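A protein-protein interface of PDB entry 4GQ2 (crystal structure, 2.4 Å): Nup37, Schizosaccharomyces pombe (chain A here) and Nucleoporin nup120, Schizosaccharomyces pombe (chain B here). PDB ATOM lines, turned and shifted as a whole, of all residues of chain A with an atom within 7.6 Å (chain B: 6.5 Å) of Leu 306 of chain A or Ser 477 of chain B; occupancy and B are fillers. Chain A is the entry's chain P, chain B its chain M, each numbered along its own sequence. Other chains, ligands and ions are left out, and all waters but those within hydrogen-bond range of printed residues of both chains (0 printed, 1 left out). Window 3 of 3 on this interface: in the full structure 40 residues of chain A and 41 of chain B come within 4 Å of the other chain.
The backbone carbonyl oxygen (O) of Ser 473 of chain B lies close to the side-chain hydroxyl (OG) of Ser 477 of chain B (3.3 Å). The backbone carbonyl oxygen of Ser 474 of chain B sits at hydrogen-bond distance from the side-chain hydroxyl of Ser 477 of chain B. The backbone carbonyl oxygen (O) of Leu 244 of chain A sits at hydrogen-bond distance from the side-chain amide nitrogen (NE2) of Gln 310 of chain A, 2.9 Å away. ND2 of Asn 304 of chain A lies close to N of Leu 306 of chain A (3.1 Å).
Leu 306 of chain A touches one residue of chain B. Of chain A, only Asn 304 and Leu 306 come within 4 Å of Ser 477 of chain B. Of the printed residues of chain A, Ser 473 of chain B touches Leu 244 (3.8 Å). Of the printed residues of chain A, Gln 480 of chain B touches Lys 303 (3.5 Å). Of the printed residues of chain A, Val 476 of chain B touches Asn 304 (3.6 Å). Of the printed residues of chain B, Leu 244 of chain A touches Leu 472 (3.9 Å) and Ser 473 (3.8 Å). The nearest residue of chain B that does not touch Leu 306 of chain A is Ser 473 of chain B (4.3 Å). The nearest printed residue of chain A that does not touch Leu 472 of chain B is Leu 306 of chain A (6.5 Å).
OD1 of Asn 304 of chain A sits close to O of Ser 477 of chain B.
Asn 240 of chain A touches Leu 472 of chain B. CB of Pro 243 of chain A touches CD2 of Leu 472 of chain B (3.8 Å). Leu 244 of chain A touches Leu 472 of chain B (CD2 to CD2, 3.9 Å). Ser 473 of chain B touches Leu 244 of chain A. Gln 480 of chain B touches Lys 303 of chain A (CA to O, 3.5 Å). Asn 304 of chain A touches Val 476 of chain B (CB to O, 3.6 Å). Asn 304 of chain A touches Ile 479 of chain B. Leu 306 of chain A touches Ser 477 of chain B.
Of the 10 printed residues of chain B, 6 touch a printed residue of chain A. Among the printed residues, 9 pairs touch across the chains.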
ATOM      1  N   LEU A 239      22.785  31.992 -13.157  1.00  0.00           N
ATOM      2  CA  LEU A 239      23.044  30.567 -13.318  1.00  0.00           C
ATOM      3  C   LEU A 239      22.233  30.113 -14.513  1.00  0.00           C
ATOM      4  O   LEU A 239      21.083  30.540 -14.692  1.00  0.00           O
ATOM      5  CB  LEU A 239      22.632  29.780 -12.068  1.00  0.00           C
ATOM      6  CG  LEU A 239      23.268  30.181 -10.734  1.00  0.00           C
ATOM      7  CD1 LEU A 239      22.523  29.565  -9.560  1.00  0.00           C
ATOM      8  CD2 LEU A 239      24.732  29.782 -10.695  1.00  0.00           C
ATOM      9  N   ASN A 240      22.834  29.279 -15.348  1.00  0.00           N
ATOM     10  CA  ASN A 240      22.154  28.768 -16.528  1.00  0.00           C
ATOM     11  C   ASN A 240      21.653  27.351 -16.257  1.00  0.00           C
ATOM     12  O   ASN A 240      22.359  26.543 -15.658  1.00  0.00           O
ATOM     13  CB  ASN A 240      23.084  28.797 -17.732  1.00  0.00           C
ATOM     14  CG  ASN A 240      23.811  30.123 -17.883  1.00  0.00           C
ATOM     15  OD1 ASN A 240      25.012  30.212 -17.615  1.00  0.00           O
ATOM     16  ND2 ASN A 240      23.090  31.161 -18.309  1.00  0.00           N
ATOM     17  N   PRO A 243      21.074  24.828 -20.765  1.00  0.00           N
ATOM     18  CA  PRO A 243      22.358  24.470 -21.377  1.00  0.00           C
ATOM     19  C   PRO A 243      23.187  23.478 -20.564  1.00  0.00           C
ATOM     20  O   PRO A 243      24.047  22.803 -21.128  1.00  0.00           O
ATOM     21  CB  PRO A 243      23.105  25.807 -21.434  1.00  0.00           C
ATOM     22  CG  PRO A 243      22.044  26.849 -21.407  1.00  0.00           C
ATOM     23  CD  PRO A 243      20.955  26.286 -20.559  1.00  0.00           C
ATOM     24  N   LEU A 244      22.939  23.396 -19.257  1.00  0.00           N
ATOM     25  CA  LEU A 244      23.758  22.567 -18.371  1.00  0.00           C
ATOM     26  C   LEU A 244      23.096  21.234 -17.985  1.00  0.00           C
ATOM     27  O   LEU A 244      23.687  20.425 -17.267  1.00  0.00           O
ATOM     28  CB  LEU A 244      24.170  23.372 -17.131  1.00  0.00           C
ATOM     29  CG  LEU A 244      24.966  24.661 -17.377  1.00  0.00           C
ATOM     30  CD1 LEU A 244      25.336  25.327 -16.067  1.00  0.00           C
ATOM     31  CD2 LEU A 244      26.221  24.408 -18.190  1.00  0.00           C
ATOM     32  N   LEU A 280      18.160  20.566 -11.181  1.00  0.00           N
ATOM     33  CA  LEU A 280      19.580  20.845 -10.894  1.00  0.00           C
ATOM     34  C   LEU A 280      19.738  21.537  -9.546  1.00  0.00           C
ATOM     35  O   LEU A 280      18.894  22.346  -9.140  1.00  0.00           O
ATOM     36  CB  LEU A 280      20.221  21.722 -11.971  1.00  0.00           C
ATOM     37  CG  LEU A 280      20.174  21.363 -13.458  1.00  0.00           C
ATOM     38  CD1 LEU A 280      18.802  21.653 -14.037  1.00  0.00           C
ATOM     39  CD2 LEU A 280      21.219  22.169 -14.210  1.00  0.00           C
ATOM     40  N   ARG A 281      20.834  21.219  -8.863  1.00  0.00           N
ATOM     41  CA  ARG A 281      21.102  21.742  -7.536  1.00  0.00           C
ATOM     42  C   ARG A 281      22.478  22.391  -7.463  1.00  0.00           C
ATOM     43  O   ARG A 281      23.476  21.776  -7.853  1.00  0.00           O
ATOM     44  CB  ARG A 281      21.030  20.609  -6.512  1.00  0.00           C
ATOM     45  CG  ARG A 281      20.664  21.067  -5.114  1.00  0.00           C
ATOM     46  CD  ARG A 281      21.530  20.412  -4.059  1.00  0.00           C
ATOM     47  NE  ARG A 281      20.765  20.112  -2.853  1.00  0.00           N
ATOM     48  CZ  ARG A 281      21.286  20.017  -1.635  1.00  0.00           C
ATOM     49  NH1 ARG A 281      22.579  20.221  -1.443  1.00  0.00           N
ATOM     50  NH2 ARG A 281      20.508  19.731  -0.602  1.00  0.00           N
ATOM     51  N   TRP A 282      22.526  23.632  -6.980  1.00  0.00           N
ATOM     52  CA  TRP A 282      23.800  24.282  -6.644  1.00  0.00           C
ATOM     53  C   TRP A 282      23.917  24.453  -5.157  1.00  0.00           C
ATOM     54  O   TRP A 282      22.968  24.884  -4.500  1.00  0.00           O
ATOM     55  CB  TRP A 282      23.914  25.663  -7.268  1.00  0.00           C
ATOM     56  CG  TRP A 282      23.996  25.718  -8.764  1.00  0.00           C
ATOM     57  CD1 TRP A 282      25.137  25.898  -9.543  1.00  0.00           C
ATOM     58  CD2 TRP A 282      22.879  25.667  -9.727  1.00  0.00           C
ATOM     59  NE1 TRP A 282      24.817  25.934 -10.878  1.00  0.00           N
ATOM     60  CE2 TRP A 282      23.479  25.803 -11.057  1.00  0.00           C
ATOM     61  CE3 TRP A 282      21.503  25.523  -9.619  1.00  0.00           C
ATOM     62  CZ2 TRP A 282      22.712  25.791 -12.217  1.00  0.00           C
ATOM     63  CZ3 TRP A 282      20.739  25.508 -10.794  1.00  0.00           C
ATOM     64  CH2 TRP A 282      21.330  25.646 -12.064  1.00  0.00           C
ATOM     65  N   ASN A 283      25.088  24.135  -4.618  1.00  0.00           N
ATOM     66  CA  ASN A 283      25.396  24.410  -3.213  1.00  0.00           C
ATOM     67  C   ASN A 283      26.268  25.649  -3.135  1.00  0.00           C
ATOM     68  O   ASN A 283      27.489  25.558  -3.037  1.00  0.00           O
ATOM     69  CB  ASN A 283      26.101  23.225  -2.563  1.00  0.00           C
ATOM     70  CG  ASN A 283      25.253  21.977  -2.551  1.00  0.00           C
ATOM     71  OD1 ASN A 283      24.057  22.017  -2.245  1.00  0.00           O
ATOM     72  ND2 ASN A 283      25.871  20.850  -2.885  1.00  0.00           N
ATOM     73  N   LYS A 303      35.352  27.083  -6.938  1.00  0.00           N
ATOM     74  CA  LYS A 303      34.725  26.217  -7.926  1.00  0.00           C
ATOM     75  C   LYS A 303      34.014  27.012  -9.015  1.00  0.00           C
ATOM     76  O   LYS A 303      33.771  28.215  -8.880  1.00  0.00           O
ATOM     77  CB  LYS A 303      33.752  25.230  -7.265  1.00  0.00           C
ATOM     78  CG  LYS A 303      34.396  24.058  -6.530  1.00  0.00           C
ATOM     79  CD  LYS A 303      35.138  23.088  -7.447  1.00  0.00           C
ATOM     80  CE  LYS A 303      36.644  23.330  -7.427  1.00  0.00           C
ATOM     81  NZ  LYS A 303      37.418  22.221  -8.049  1.00  0.00           N
ATOM     82  N   ASN A 304      33.696  26.323 -10.104  1.00  0.00           N
ATOM     83  CA  ASN A 304      32.901  26.907 -11.156  1.00  0.00           C
ATOM     84  C   ASN A 304      31.410  26.883 -10.776  1.00  0.00           C
ATOM     85  O   ASN A 304      31.046  26.408  -9.695  1.00  0.00           O
ATOM     86  CB  ASN A 304      33.193  26.212 -12.489  1.00  0.00           C
ATOM     87  CG  ASN A 304      32.860  24.731 -12.471  1.00  0.00           C
ATOM     88  OD1 ASN A 304      33.559  23.923 -13.084  1.00  0.00           O
ATOM     89  ND2 ASN A 304      31.778  24.371 -11.795  1.00  0.00           N
ATOM     90  N   LEU A 305      30.556  27.402 -11.655  1.00  0.00           N
ATOM     91  CA  LEU A 305      29.131  27.507 -11.353  1.00  0.00           C
ATOM     92  C   LEU A 305      28.281  26.420 -12.008  1.00  0.00           C
ATOM     93  O   LEU A 305      27.076  26.592 -12.203  1.00  0.00           O
ATOM     94  CB  LEU A 305      28.620  28.903 -11.712  1.00  0.00           C
ATOM     95  CG  LEU A 305      28.356  29.889 -10.570  1.00  0.00           C
ATOM     96  CD1 LEU A 305      29.358  29.794  -9.434  1.00  0.00           C
ATOM     97  CD2 LEU A 305      28.313  31.296 -11.132  1.00  0.00           C
ATOM     98  N   LEU A 306      28.913  25.306 -12.355  1.00  0.00           N
ATOM     99  CA  LEU A 306      28.183  24.132 -12.788  1.00  0.00           C
ATOM    100  C   LEU A 306      27.390  23.608 -11.595  1.00  0.00           C
ATOM    101  O   LEU A 306      27.858  23.690 -10.459  1.00  0.00           O
ATOM    102  CB  LEU A 306      29.139  23.051 -13.297  1.00  0.00           C
ATOM    103  CG  LEU A 306      29.953  23.257 -14.582  1.00  0.00           C
ATOM    104  CD1 LEU A 306      31.007  22.166 -14.698  1.00  0.00           C
ATOM    105  CD2 LEU A 306      29.085  23.254 -15.827  1.00  0.00           C
ATOM    106  N   PRO A 307      26.185  23.067 -11.842  1.00  0.00           N
ATOM    107  CA  PRO A 307      25.454  22.450 -10.738  1.00  0.00           C
ATOM    108  C   PRO A 307      26.287  21.355 -10.082  1.00  0.00           C
ATOM    109  O   PRO A 307      27.113  20.716 -10.741  1.00  0.00           O
ATOM    110  CB  PRO A 307      24.218  21.848 -11.422  1.00  0.00           C
ATOM    111  CG  PRO A 307      24.610  21.686 -12.855  1.00  0.00           C
ATOM    112  CD  PRO A 307      25.503  22.861 -13.135  1.00  0.00           C
ATOM    113  N   ASN A 308      26.084  21.160  -8.787  1.00  0.00           N
ATOM    114  CA  ASN A 308      26.846  20.171  -8.037  1.00  0.00           C
ATOM    115  C   ASN A 308      26.325  18.760  -8.284  1.00  0.00           C
ATOM    116  O   ASN A 308      27.102  17.813  -8.401  1.00  0.00           O
ATOM    117  CB  ASN A 308      26.831  20.527  -6.552  1.00  0.00           C
ATOM    118  CG  ASN A 308      27.483  21.873  -6.280  1.00  0.00           C
ATOM    119  OD1 ASN A 308      26.807  22.856  -5.989  1.00  0.00           O
ATOM    120  ND2 ASN A 308      28.805  21.931  -6.418  1.00  0.00           N
ATOM    121  N   VAL A 309      25.003  18.646  -8.384  1.00  0.00           N
ATOM    122  CA  VAL A 309      24.335  17.389  -8.681  1.00  0.00           C
ATOM    123  C   VAL A 309      23.075  17.693  -9.495  1.00  0.00           C
ATOM    124  O   VAL A 309      22.487  18.766  -9.367  1.00  0.00           O
ATOM    125  CB  VAL A 309      24.003  16.607  -7.381  1.00  0.00           C
ATOM    126  CG1 VAL A 309      22.905  17.294  -6.581  1.00  0.00           C
ATOM    127  CG2 VAL A 309      23.628  15.164  -7.680  1.00  0.00           C
ATOM    128  N   GLN A 310      22.685  16.762 -10.356  1.00  0.00           N
ATOM    129  CA  GLN A 310      21.421  16.879 -11.072  1.00  0.00           C
ATOM    130  C   GLN A 310      20.809  15.520 -11.365  1.00  0.00           C
ATOM    131  O   GLN A 310      21.483  14.499 -11.325  1.00  0.00           O
ATOM    132  CB  GLN A 310      21.569  17.699 -12.364  1.00  0.00           C
ATOM    133  CG  GLN A 310      22.604  17.187 -13.341  1.00  0.00           C
ATOM    134  CD  GLN A 310      22.597  17.967 -14.642  1.00  0.00           C
ATOM    135  OE1 GLN A 310      21.724  17.773 -15.479  1.00  0.00           O
ATOM    136  NE2 GLN A 310      23.591  18.834 -14.830  1.00  0.00           N
ATOM    137  N   PHE B 444      39.414  24.735 -26.455  1.00  0.00           N
ATOM    138  CA  PHE B 444      38.976  25.104 -25.104  1.00  0.00           C
ATOM    139  C   PHE B 444      38.706  23.862 -24.252  1.00  0.00           C
ATOM    140  O   PHE B 444      37.963  23.912 -23.267  1.00  0.00           O
ATOM    141  CB  PHE B 444      37.759  26.050 -25.162  1.00  0.00           C
ATOM    142  CG  PHE B 444      38.126  27.508 -25.316  1.00  0.00           C
ATOM    143  CD1 PHE B 444      38.977  27.933 -26.345  1.00  0.00           C
ATOM    144  CD2 PHE B 444      37.621  28.465 -24.437  1.00  0.00           C
ATOM    145  CE1 PHE B 444      39.322  29.272 -26.483  1.00  0.00           C
ATOM    146  CE2 PHE B 444      37.958  29.809 -24.576  1.00  0.00           C
ATOM    147  CZ  PHE B 444      38.811  30.211 -25.597  1.00  0.00           C
ATOM    148  N   LEU B 472      28.629  26.924 -24.216  1.00  0.00           N
ATOM    149  CA  LEU B 472      28.328  27.592 -22.958  1.00  0.00           C
ATOM    150  C   LEU B 472      28.868  26.795 -21.775  1.00  0.00           C
ATOM    151  O   LEU B 472      29.495  27.354 -20.869  1.00  0.00           O
ATOM    152  CB  LEU B 472      26.820  27.836 -22.788  1.00  0.00           C
ATOM    153  CG  LEU B 472      26.403  28.594 -21.509  1.00  0.00           C
ATOM    154  CD1 LEU B 472      25.122  29.393 -21.706  1.00  0.00           C
ATOM    155  CD2 LEU B 472      26.263  27.671 -20.305  1.00  0.00           C
ATOM    156  N   SER B 473      28.597  25.492 -21.787  1.00  0.00           N
ATOM    157  CA  SER B 473      29.017  24.607 -20.709  1.00  0.00           C
ATOM    158  C   SER B 473      30.524  24.646 -20.501  1.00  0.00           C
ATOM    159  O   SER B 473      30.988  24.739 -19.375  1.00  0.00           O
ATOM    160  CB  SER B 473      28.561  23.172 -20.976  1.00  0.00           C
ATOM    161  OG  SER B 473      29.091  22.296 -20.005  1.00  0.00           O
ATOM    162  N   SER B 474      31.283  24.578 -21.588  1.00  0.00           N
ATOM    163  CA  SER B 474      32.732  24.504 -21.482  1.00  0.00           C
ATOM    164  C   SER B 474      33.365  25.827 -21.024  1.00  0.00           C
ATOM    165  O   SER B 474      34.387  25.815 -20.342  1.00  0.00           O
ATOM    166  CB  SER B 474      33.348  24.024 -22.795  1.00  0.00           C
ATOM    167  OG  SER B 474      33.312  25.042 -23.771  1.00  0.00           O
ATOM    168  N   ILE B 475      32.766  26.957 -21.400  1.00  0.00           N
ATOM    169  CA  ILE B 475      33.213  28.264 -20.908  1.00  0.00           C
ATOM    170  C   ILE B 475      32.852  28.481 -19.436  1.00  0.00           C
ATOM    171  O   ILE B 475      33.691  28.926 -18.649  1.00  0.00           O
ATOM    172  CB  ILE B 475      32.682  29.412 -21.784  1.00  0.00           C
ATOM    173  CG1 ILE B 475      33.617  29.605 -22.969  1.00  0.00           C
ATOM    174  CG2 ILE B 475      32.602  30.719 -21.000  1.00  0.00           C
ATOM    175  CD1 ILE B 475      32.917  30.090 -24.212  1.00  0.00           C
ATOM    176  N   VAL B 476      31.614  28.145 -19.069  1.00  0.00           N
ATOM    177  CA  VAL B 476      31.143  28.287 -17.684  1.00  0.00           C
ATOM    178  C   VAL B 476      31.948  27.395 -16.728  1.00  0.00           C
ATOM    179  O   VAL B 476      32.180  27.764 -15.584  1.00  0.00           O
ATOM    180  CB  VAL B 476      29.608  28.061 -17.578  1.00  0.00           C
ATOM    181  CG1 VAL B 476      29.131  27.998 -16.131  1.00  0.00           C
ATOM    182  CG2 VAL B 476      28.878  29.185 -18.292  1.00  0.00           C
ATOM    183  N   SER B 477      32.403  26.244 -17.216  1.00  0.00           N
ATOM    184  CA  SER B 477      33.155  25.287 -16.397  1.00  0.00           C
ATOM    185  C   SER B 477      34.597  25.719 -16.106  1.00  0.00           C
ATOM    186  O   SER B 477      35.182  25.276 -15.130  1.00  0.00           O
ATOM    187  CB  SER B 477      33.159  23.910 -17.060  1.00  0.00           C
ATOM    188  OG  SER B 477      33.967  23.929 -18.219  1.00  0.00           O
ATOM    189  N   THR B 478      35.166  26.572 -16.955  1.00  0.00           N
ATOM    190  CA  THR B 478      36.542  27.028 -16.759  1.00  0.00           C
ATOM    191  C   THR B 478      36.644  28.219 -15.817  1.00  0.00           C
ATOM    192  O   THR B 478      37.727  28.526 -15.324  1.00  0.00           O
ATOM    193  CB  THR B 478      37.248  27.407 -18.086  1.00  0.00           C
ATOM    194  OG1 THR B 478      36.494  28.412 -18.775  1.00  0.00           O
ATOM    195  CG2 THR B 478      37.431  26.195 -18.984  1.00  0.00           C
ATOM    196  N   ILE B 479      35.529  28.899 -15.570  1.00  0.00           N
ATOM    197  CA  ILE B 479      35.578  30.142 -14.801  1.00  0.00           C
ATOM    198  C   ILE B 479      35.151  29.935 -13.357  1.00  0.00           C
ATOM    199  O   ILE B 479      34.047  29.474 -13.081  1.00  0.00           O
ATOM    200  CB  ILE B 479      34.773  31.281 -15.474  1.00  0.00           C
ATOM    201  CG1 ILE B 479      35.110  31.379 -16.972  1.00  0.00           C
ATOM    202  CG2 ILE B 479      35.034  32.608 -14.780  1.00  0.00           C
ATOM    203  CD1 ILE B 479      36.593  31.483 -17.290  1.00  0.00           C
ATOM    204  N   GLN B 480      36.042  30.287 -12.438  1.00  0.00           N
ATOM    205  CA  GLN B 480      35.829  30.028 -11.021  1.00  0.00           C
ATOM    206  C   GLN B 480      35.419  31.288 -10.280  1.00  0.00           C
ATOM    207  O   GLN B 480      35.961  32.363 -10.520  1.00  0.00           O
ATOM    208  CB  GLN B 480      37.092  29.430 -10.396  1.00  0.00           C
ATOM    209  CG  GLN B 480      37.508  28.096 -11.004  1.00  0.00           C
ATOM    210  CD  GLN B 480      38.783  27.535 -10.402  1.00  0.00           C
ATOM    211  OE1 GLN B 480      39.423  28.163  -9.550  1.00  0.00           O
ATOM    212  NE2 GLN B 480      39.161  26.340 -10.843  1.00  0.00           N
